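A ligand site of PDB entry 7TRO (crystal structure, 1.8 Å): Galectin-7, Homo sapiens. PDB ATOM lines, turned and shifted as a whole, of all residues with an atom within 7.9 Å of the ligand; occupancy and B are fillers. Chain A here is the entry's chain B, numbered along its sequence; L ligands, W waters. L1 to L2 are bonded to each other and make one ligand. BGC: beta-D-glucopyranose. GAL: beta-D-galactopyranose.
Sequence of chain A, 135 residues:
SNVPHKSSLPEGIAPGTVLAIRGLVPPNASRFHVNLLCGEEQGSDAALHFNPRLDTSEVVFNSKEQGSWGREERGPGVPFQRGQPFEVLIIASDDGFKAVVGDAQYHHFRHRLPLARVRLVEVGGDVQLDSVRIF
O6 of GAL L2 lies within hydrogen-bond range of OE2 of Glu 72, at 2.7 Å.
O4 of GAL L2 is in hydrogen-bond range of NE2 of His 49 (2.8 Å).
An oxygen (O3) of BGC L1 is in hydrogen-bond range of the guanidinium group (NH1) of Arg 53.
The side-chain amide oxygen (OD1) of Asn 51 lies within hydrogen-bond range of an oxygen (O4) of GAL L2.
ND2 of Asn 62 sits at hydrogen-bond distance from O6 of GAL L2.
An oxygen (O3) of BGC L1 sits at hydrogen-bond distance from the guanidinium group (NH2) of Arg 74, at 3.5 Å.
The guanidinium group of Arg 74 is in salt-bridge range of the side-chain carboxylate of Glu 72, 3.4 Å away.
NE of Arg 53 is in hydrogen-bond range of OD1 of Asn 51, at 2.7 Å.
The guanidinium group (NH1) of Arg 53 is in salt-bridge range of the side-chain carboxylate (OE1) of Glu 58 (3.0 Å).
The backbone NH (N) of Asn 51 sits at hydrogen-bond distance from the backbone carbonyl oxygen (O) of Val 60, at 2.8 Å.
ND2 of Asn 51 lies within hydrogen-bond range of O of Phe 32, at 2.7 Å.
The backbone carbonyl oxygen (O) of Gly 70 sits at hydrogen-bond distance from the side-chain amide nitrogen (ND2) of Asn 62, 2.9 Å away.
The side-chain amide oxygen (OD1) of Asn 62 sits close to the backbone carbonyl oxygen (O) of Arg 71.
NE of Arg 74 is in salt-bridge range of OE2 of Glu 58 (3.1 Å).
Merely in contact with the ligand: Val 60 (3.9 Å) and Trp 69 (3.8 Å).
Hydrophobic or aromatic side chains that line the ligand: His 49, Val 60 and Trp 69.
Within 4 Å of the ligand: His 49, Asn 51, Arg 53, Val 60, Asn 62, Trp 69, Glu 72 and Arg 74.
Water W2 bridges the side-chain amide oxygen of Asn 51 (2.8 Å) and an oxygen (O4) of GAL L2 (2.9 Å).
Water W1 bridges NH1 of Arg 31 (2.5 Å) and O2 of GAL L2 (3.3 Å).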
ATOM      1  N   ARG A  31      -5.011  21.721 -15.089  1.00  0.00           N
ATOM      2  CA  ARG A  31      -4.110  22.267 -14.086  1.00  0.00           C
ATOM      3  C   ARG A  31      -2.775  21.578 -14.242  1.00  0.00           C
ATOM      4  O   ARG A  31      -2.703  20.460 -14.754  1.00  0.00           O
ATOM      5  CB  ARG A  31      -4.674  22.068 -12.670  1.00  0.00           C
ATOM      6  CG  ARG A  31      -5.223  20.676 -12.393  1.00  0.00           C
ATOM      7  CD  ARG A  31      -5.963  20.593 -11.035  1.00  0.00           C
ATOM      8  NE  ARG A  31      -7.063  21.551 -10.954  1.00  0.00           N
ATOM      9  CZ  ARG A  31      -7.803  21.753  -9.878  1.00  0.00           C
ATOM     10  NH1 ARG A  31      -7.586  21.089  -8.749  1.00  0.00           N
ATOM     11  NH2 ARG A  31      -8.803  22.628  -9.924  1.00  0.00           N
ATOM     12  N   PHE A  32      -1.703  22.282 -13.832  1.00  0.00           N
ATOM     13  CA  PHE A  32      -0.379  21.679 -13.727  1.00  0.00           C
ATOM     14  C   PHE A  32       0.283  22.238 -12.491  1.00  0.00           C
ATOM     15  O   PHE A  32      -0.249  23.141 -11.845  1.00  0.00           O
ATOM     16  CB  PHE A  32       0.504  21.916 -14.949  1.00  0.00           C
ATOM     17  CG  PHE A  32       0.954  23.337 -15.126  1.00  0.00           C
ATOM     18  CD1 PHE A  32       0.114  24.286 -15.674  1.00  0.00           C
ATOM     19  CD2 PHE A  32       2.259  23.717 -14.800  1.00  0.00           C
ATOM     20  CE1 PHE A  32       0.542  25.592 -15.866  1.00  0.00           C
ATOM     21  CE2 PHE A  32       2.687  25.001 -14.990  1.00  0.00           C
ATOM     22  CZ  PHE A  32       1.824  25.947 -15.529  1.00  0.00           C
ATOM     23  N   HIS A  33       1.435  21.679 -12.130  1.00  0.00           N
ATOM     24  CA  HIS A  33       2.058  22.041 -10.872  1.00  0.00           C
ATOM     25  C   HIS A  33       3.559  21.845 -10.955  1.00  0.00           C
ATOM     26  O   HIS A  33       4.055  21.062 -11.756  1.00  0.00           O
ATOM     27  CB  HIS A  33       1.479  21.218  -9.721  1.00  0.00           C
ATOM     28  CG  HIS A  33       1.690  19.758  -9.882  1.00  0.00           C
ATOM     29  ND1 HIS A  33       0.721  18.922 -10.421  1.00  0.00           N
ATOM     30  CD2 HIS A  33       2.755  18.964  -9.624  1.00  0.00           C
ATOM     31  CE1 HIS A  33       1.185  17.690 -10.477  1.00  0.00           C
ATOM     32  NE2 HIS A  33       2.414  17.679  -9.994  1.00  0.00           N
ATOM     33  N   ASN A  35       6.552  20.991  -8.077  1.00  0.00           N
ATOM     34  CA  ASN A  35       6.768  20.609  -6.680  1.00  0.00           C
ATOM     35  C   ASN A  35       8.249  20.641  -6.376  1.00  0.00           C
ATOM     36  O   ASN A  35       9.075  20.180  -7.188  1.00  0.00           O
ATOM     37  CB  ASN A  35       6.226  19.201  -6.352  1.00  0.00           C
ATOM     38  CG  ASN A  35       4.708  19.137  -6.359  1.00  0.00           C
ATOM     39  OD1 ASN A  35       4.021  20.149  -6.243  1.00  0.00           O
ATOM     40  ND2 ASN A  35       4.177  17.920  -6.495  1.00  0.00           N
ATOM     41  N   HIS A  49       4.611  23.670  -3.400  1.00  0.00           N
ATOM     42  CA  HIS A  49       3.706  23.165  -4.433  1.00  0.00           C
ATOM     43  C   HIS A  49       3.118  24.403  -5.078  1.00  0.00           C
ATOM     44  O   HIS A  49       2.419  25.186  -4.411  1.00  0.00           O
ATOM     45  CB  HIS A  49       2.616  22.262  -3.802  1.00  0.00           C
ATOM     46  CG  HIS A  49       1.489  21.874  -4.718  1.00  0.00           C
ATOM     47  ND1 HIS A  49       1.613  20.898  -5.685  1.00  0.00           N
ATOM     48  CD2 HIS A  49       0.196  22.278  -4.753  1.00  0.00           C
ATOM     49  CE1 HIS A  49       0.448  20.731  -6.302  1.00  0.00           C
ATOM     50  NE2 HIS A  49      -0.427  21.564  -5.758  1.00  0.00           N
ATOM     51  N   PHE A  50       3.419  24.611  -6.366  1.00  0.00           N
ATOM     52  CA  PHE A  50       2.983  25.735  -7.176  1.00  0.00           C
ATOM     53  C   PHE A  50       2.035  25.196  -8.234  1.00  0.00           C
ATOM     54  O   PHE A  50       2.475  24.478  -9.148  1.00  0.00           O
ATOM     55  CB  PHE A  50       4.207  26.397  -7.802  1.00  0.00           C
ATOM     56  CG  PHE A  50       3.916  27.388  -8.864  1.00  0.00           C
ATOM     57  CD1 PHE A  50       3.471  28.641  -8.530  1.00  0.00           C
ATOM     58  CD2 PHE A  50       4.146  27.090 -10.188  1.00  0.00           C
ATOM     59  CE1 PHE A  50       3.229  29.582  -9.494  1.00  0.00           C
ATOM     60  CE2 PHE A  50       3.901  28.006 -11.173  1.00  0.00           C
ATOM     61  CZ  PHE A  50       3.454  29.273 -10.837  1.00  0.00           C
ATOM     62  N   ASN A  51       0.757  25.559  -8.163  1.00  0.00           N
ATOM     63  CA  ASN A  51      -0.319  24.846  -8.866  1.00  0.00           C
ATOM     64  C   ASN A  51      -1.221  25.798  -9.646  1.00  0.00           C
ATOM     65  O   ASN A  51      -2.278  26.206  -9.166  1.00  0.00           O
ATOM     66  CB  ASN A  51      -1.105  24.010  -7.868  1.00  0.00           C
ATOM     67  CG  ASN A  51      -2.191  23.169  -8.512  1.00  0.00           C
ATOM     68  OD1 ASN A  51      -3.178  22.821  -7.855  1.00  0.00           O
ATOM     69  ND2 ASN A  51      -2.024  22.850  -9.790  1.00  0.00           N
ATOM     70  N   ARG A  53      -4.138  26.674 -11.993  1.00  0.00           N
ATOM     71  CA  ARG A  53      -5.380  25.942 -12.222  1.00  0.00           C
ATOM     72  C   ARG A  53      -6.218  26.701 -13.250  1.00  0.00           C
ATOM     73  O   ARG A  53      -6.828  27.722 -12.919  1.00  0.00           O
ATOM     74  CB  ARG A  53      -6.149  25.747 -10.932  1.00  0.00           C
ATOM     75  CG  ARG A  53      -5.438  24.868  -9.947  1.00  0.00           C
ATOM     76  CD  ARG A  53      -6.172  24.933  -8.638  1.00  0.00           C
ATOM     77  NE  ARG A  53      -5.600  24.045  -7.638  1.00  0.00           N
ATOM     78  CZ  ARG A  53      -6.110  23.883  -6.431  1.00  0.00           C
ATOM     79  NH1 ARG A  53      -7.194  24.554  -6.051  1.00  0.00           N
ATOM     80  NH2 ARG A  53      -5.494  23.070  -5.569  1.00  0.00           N
ATOM     81  N   THR A  56     -10.359  26.231 -12.434  1.00  0.00           N
ATOM     82  CA  THR A  56     -10.876  27.101 -11.374  1.00  0.00           C
ATOM     83  C   THR A  56     -10.290  28.506 -11.400  1.00  0.00           C
ATOM     84  O   THR A  56     -10.552  29.287 -10.465  1.00  0.00           O
ATOM     85  CB  THR A  56     -10.591  26.478 -10.003  1.00  0.00           C
ATOM     86  OG1 THR A  56      -9.194  26.181  -9.911  1.00  0.00           O
ATOM     87  CG2 THR A  56     -11.396  25.205  -9.796  1.00  0.00           C
ATOM     88  N   GLU A  58      -7.374  29.802 -10.824  1.00  0.00           N
ATOM     89  CA  GLU A  58      -6.704  29.956  -9.546  1.00  0.00           C
ATOM     90  C   GLU A  58      -5.212  29.701  -9.741  1.00  0.00           C
ATOM     91  O   GLU A  58      -4.807  29.015 -10.686  1.00  0.00           O
ATOM     92  CB  GLU A  58      -7.252  28.928  -8.557  1.00  0.00           C
ATOM     93  CG  GLU A  58      -8.235  29.416  -7.549  1.00  0.00           C
ATOM     94  CD  GLU A  58      -8.800  28.257  -6.749  1.00  0.00           C
ATOM     95  OE1 GLU A  58      -8.398  27.079  -7.010  1.00  0.00           O
ATOM     96  OE2 GLU A  58      -9.651  28.503  -5.885  1.00  0.00           O
ATOM     97  N   VAL A  60      -2.560  28.210  -6.841  1.00  0.00           N
ATOM     98  CA  VAL A  60      -2.502  27.743  -5.457  1.00  0.00           C
ATOM     99  C   VAL A  60      -1.059  27.438  -5.109  1.00  0.00           C
ATOM    100  O   VAL A  60      -0.327  26.817  -5.889  1.00  0.00           O
ATOM    101  CB  VAL A  60      -3.390  26.500  -5.220  1.00  0.00           C
ATOM    102  CG1 VAL A  60      -3.084  25.841  -3.882  1.00  0.00           C
ATOM    103  CG2 VAL A  60      -4.883  26.867  -5.314  1.00  0.00           C
ATOM    104  N   PHE A  61      -0.636  27.905  -3.932  1.00  0.00           N
ATOM    105  CA  PHE A  61       0.653  27.570  -3.346  1.00  0.00           C
ATOM    106  C   PHE A  61       0.393  26.836  -2.049  1.00  0.00           C
ATOM    107  O   PHE A  61      -0.489  27.214  -1.284  1.00  0.00           O
ATOM    108  CB  PHE A  61       1.477  28.817  -3.032  1.00  0.00           C
ATOM    109  CG  PHE A  61       1.751  29.674  -4.209  1.00  0.00           C
ATOM    110  CD1 PHE A  61       0.729  30.385  -4.810  1.00  0.00           C
ATOM    111  CD2 PHE A  61       3.018  29.789  -4.711  1.00  0.00           C
ATOM    112  CE1 PHE A  61       0.999  31.200  -5.886  1.00  0.00           C
ATOM    113  CE2 PHE A  61       3.280  30.621  -5.762  1.00  0.00           C
ATOM    114  CZ  PHE A  61       2.271  31.304  -6.366  1.00  0.00           C
ATOM    115  N   ASN A  62       1.176  25.819  -1.783  1.00  0.00           N
ATOM    116  CA  ASN A  62       0.990  25.116  -0.535  1.00  0.00           C
ATOM    117  C   ASN A  62       2.249  24.339  -0.231  1.00  0.00           C
ATOM    118  O   ASN A  62       3.200  24.309  -1.000  1.00  0.00           O
ATOM    119  CB  ASN A  62      -0.263  24.195  -0.576  1.00  0.00           C
ATOM    120  CG  ASN A  62      -0.882  23.957   0.825  1.00  0.00           C
ATOM    121  OD1 ASN A  62      -0.214  24.148   1.864  1.00  0.00           O
ATOM    122  ND2 ASN A  62      -2.145  23.558   0.849  1.00  0.00           N
ATOM    123  N   SER A  63       2.234  23.755   0.937  1.00  0.00           N
ATOM    124  CA  SER A  63       3.264  22.872   1.422  1.00  0.00           C
ATOM    125  C   SER A  63       2.587  21.569   1.774  1.00  0.00           C
ATOM    126  O   SER A  63       1.353  21.521   1.903  1.00  0.00           O
ATOM    127  CB  SER A  63       3.943  23.459   2.668  1.00  0.00           C
ATOM    128  OG  SER A  63       2.906  23.867   3.578  1.00  0.00           O
ATOM    129  N   LYS A  64       3.382  20.511   1.922  1.00  0.00           N
ATOM    130  CA  LYS A  64       2.839  19.192   2.239  1.00  0.00           C
ATOM    131  C   LYS A  64       3.793  18.521   3.204  1.00  0.00           C
ATOM    132  O   LYS A  64       4.985  18.416   2.905  1.00  0.00           O
ATOM    133  CB  LYS A  64       2.658  18.296   1.002  1.00  0.00           C
ATOM    134  CG  LYS A  64       1.709  17.070   1.235  1.00  0.00           C
ATOM    135  CD  LYS A  64       1.420  16.250  -0.036  1.00  0.00           C
ATOM    136  CE  LYS A  64       2.634  15.410  -0.487  1.00  0.00           C
ATOM    137  NZ  LYS A  64       2.367  14.661  -1.775  1.00  0.00           N
ATOM    138  N   TRP A  69      -1.773  18.306   3.337  1.00  0.00           N
ATOM    139  CA  TRP A  69      -1.574  19.628   2.717  1.00  0.00           C
ATOM    140  C   TRP A  69      -1.733  20.694   3.799  1.00  0.00           C
ATOM    141  O   TRP A  69      -2.561  20.489   4.692  1.00  0.00           O
ATOM    142  CB  TRP A  69      -2.518  19.868   1.513  1.00  0.00           C
ATOM    143  CG  TRP A  69      -2.200  18.978   0.346  1.00  0.00           C
ATOM    144  CD1 TRP A  69      -2.844  17.841  -0.040  1.00  0.00           C
ATOM    145  CD2 TRP A  69      -1.123  19.163  -0.584  1.00  0.00           C
ATOM    146  NE1 TRP A  69      -2.243  17.316  -1.162  1.00  0.00           N
ATOM    147  CE2 TRP A  69      -1.181  18.105  -1.512  1.00  0.00           C
ATOM    148  CE3 TRP A  69      -0.134  20.130  -0.728  1.00  0.00           C
ATOM    149  CZ2 TRP A  69      -0.286  17.993  -2.566  1.00  0.00           C
ATOM    150  CZ3 TRP A  69       0.767  20.030  -1.764  1.00  0.00           C
ATOM    151  CH2 TRP A  69       0.695  18.968  -2.681  1.00  0.00           C
ATOM    152  N   GLY A  70      -0.966  21.785   3.730  1.00  0.00           N
ATOM    153  CA  GLY A  70      -1.033  22.905   4.653  1.00  0.00           C
ATOM    154  C   GLY A  70      -2.121  23.888   4.295  1.00  0.00           C
ATOM    155  O   GLY A  70      -3.077  23.572   3.580  1.00  0.00           O
ATOM    156  N   ARG A  71      -1.957  25.125   4.796  1.00  0.00           N
ATOM    157  CA  ARG A  71      -2.841  26.223   4.469  1.00  0.00           C
ATOM    158  C   ARG A  71      -2.533  26.736   3.063  1.00  0.00           C
ATOM    159  O   ARG A  71      -1.392  27.104   2.763  1.00  0.00           O
ATOM    160  CB  ARG A  71      -2.702  27.377   5.468  1.00  0.00           C
ATOM    161  CG  ARG A  71      -3.698  28.518   5.204  1.00  0.00           C
ATOM    162  CD  ARG A  71      -3.493  29.688   6.148  1.00  0.00           C
ATOM    163  NE  ARG A  71      -2.216  30.384   5.938  1.00  0.00           N
ATOM    164  CZ  ARG A  71      -1.970  31.299   5.012  1.00  0.00           C
ATOM    165  NH1 ARG A  71      -2.915  31.715   4.173  1.00  0.00           N
ATOM    166  NH2 ARG A  71      -0.754  31.832   4.945  1.00  0.00           N
ATOM    167  N   GLU A  72      -3.573  26.799   2.251  1.00  0.00           N
ATOM    168  CA  GLU A  72      -3.411  27.236   0.866  1.00  0.00           C
ATOM    169  C   GLU A  72      -3.217  28.746   0.814  1.00  0.00           C
ATOM    170  O   GLU A  72      -3.851  29.432   1.604  1.00  0.00           O
ATOM    171  CB  GLU A  72      -4.623  26.883  -0.012  1.00  0.00           C
ATOM    172  CG  GLU A  72      -4.712  25.379  -0.282  1.00  0.00           C
ATOM    173  CD  GLU A  72      -5.929  25.050  -1.141  1.00  0.00           C
ATOM    174  OE1 GLU A  72      -7.034  25.442  -0.751  1.00  0.00           O
ATOM    175  OE2 GLU A  72      -5.765  24.451  -2.204  1.00  0.00           O
ATOM    176  N   GLU A  73      -2.294  29.200  -0.008  1.00  0.00           N
ATOM    177  CA  GLU A  73      -2.144  30.593  -0.379  1.00  0.00           C
ATOM    178  C   GLU A  73      -2.463  30.712  -1.852  1.00  0.00           C
ATOM    179  O   GLU A  73      -2.269  29.763  -2.617  1.00  0.00           O
ATOM    180  CB  GLU A  73      -0.695  31.107  -0.152  1.00  0.00           C
ATOM    181  CG  GLU A  73      -0.242  31.105   1.305  1.00  0.00           C
ATOM    182  CD  GLU A  73       1.221  31.489   1.463  1.00  0.00           C
ATOM    183  OE1 GLU A  73       1.709  32.340   0.689  1.00  0.00           O
ATOM    184  OE2 GLU A  73       1.900  30.891   2.321  1.00  0.00           O
ATOM    185  N   ARG A  74      -2.936  31.887  -2.258  1.00  0.00           N
ATOM    186  CA  ARG A  74      -3.276  32.152  -3.637  1.00  0.00           C
ATOM    187  C   ARG A  74      -2.674  33.468  -4.096  1.00  0.00           C
ATOM    188  O   ARG A  74      -2.732  34.462  -3.383  1.00  0.00           O
ATOM    189  CB  ARG A  74      -4.808  32.212  -3.845  1.00  0.00           C
ATOM    190  CG  ARG A  74      -5.488  30.850  -3.938  1.00  0.00           C
ATOM    191  CD  ARG A  74      -6.980  30.925  -3.595  1.00  0.00           C
ATOM    192  NE  ARG A  74      -7.603  29.625  -3.839  1.00  0.00           N
ATOM    193  CZ  ARG A  74      -7.555  28.600  -2.988  1.00  0.00           C
ATOM    194  NH1 ARG A  74      -7.044  28.722  -1.773  1.00  0.00           N
ATOM    195  NH2 ARG A  74      -8.033  27.420  -3.370  1.00  0.00           N
HETATM  196  C2  BGC L   1     -10.157  22.444  -3.504  1.00  0.00           C
HETATM  197  C3  BGC L   1      -8.639  22.576  -3.780  1.00  0.00           C
HETATM  198  C4  BGC L   1      -7.770  21.478  -3.048  1.00  0.00           C
HETATM  199  C5  BGC L   1      -8.492  20.657  -1.903  1.00  0.00           C
HETATM  200  C6  BGC L   1      -7.678  20.653  -0.562  1.00  0.00           C
HETATM  201  C1  BGC L   1     -10.358  22.316  -1.980  1.00  0.00           C
HETATM  202  O1  BGC L   1      -9.713  23.333  -1.187  1.00  0.00           O
HETATM  203  O2  BGC L   1     -10.694  21.321  -4.254  1.00  0.00           O
HETATM  204  O3  BGC L   1      -8.255  23.948  -3.470  1.00  0.00           O
HETATM  205  O4  BGC L   1      -7.144  20.555  -4.002  1.00  0.00           O
HETATM  206  O5  BGC L   1      -9.832  21.066  -1.569  1.00  0.00           O
HETATM  207  O6  BGC L   1      -8.217  19.782   0.447  1.00  0.00           O
HETATM  208  C1  GAL L   2      -5.894  19.906  -3.688  1.00  0.00           C
HETATM  209  C2  GAL L   2      -5.342  19.117  -4.893  1.00  0.00           C
HETATM  210  C3  GAL L   2      -3.866  18.683  -4.646  1.00  0.00           C
HETATM  211  C4  GAL L   2      -3.036  19.920  -4.273  1.00  0.00           C
HETATM  212  C5  GAL L   2      -3.603  20.569  -3.027  1.00  0.00           C
HETATM  213  C6  GAL L   2      -2.900  21.882  -2.581  1.00  0.00           C
HETATM  214  O2  GAL L   2      -6.197  17.993  -5.226  1.00  0.00           O
HETATM  215  O3  GAL L   2      -3.247  18.009  -5.773  1.00  0.00           O
HETATM  216  O4  GAL L   2      -3.072  20.903  -5.317  1.00  0.00           O
HETATM  217  O5  GAL L   2      -4.951  20.915  -3.312  1.00  0.00           O
HETATM  218  O6  GAL L   2      -3.790  22.648  -1.772  1.00  0.00           O
HETATM  219  O   HOH W   1      -6.214  19.055  -8.387  1.00  0.00           O
HETATM  220  O   HOH W   2      -3.419  20.088  -8.129  1.00  0.00           O
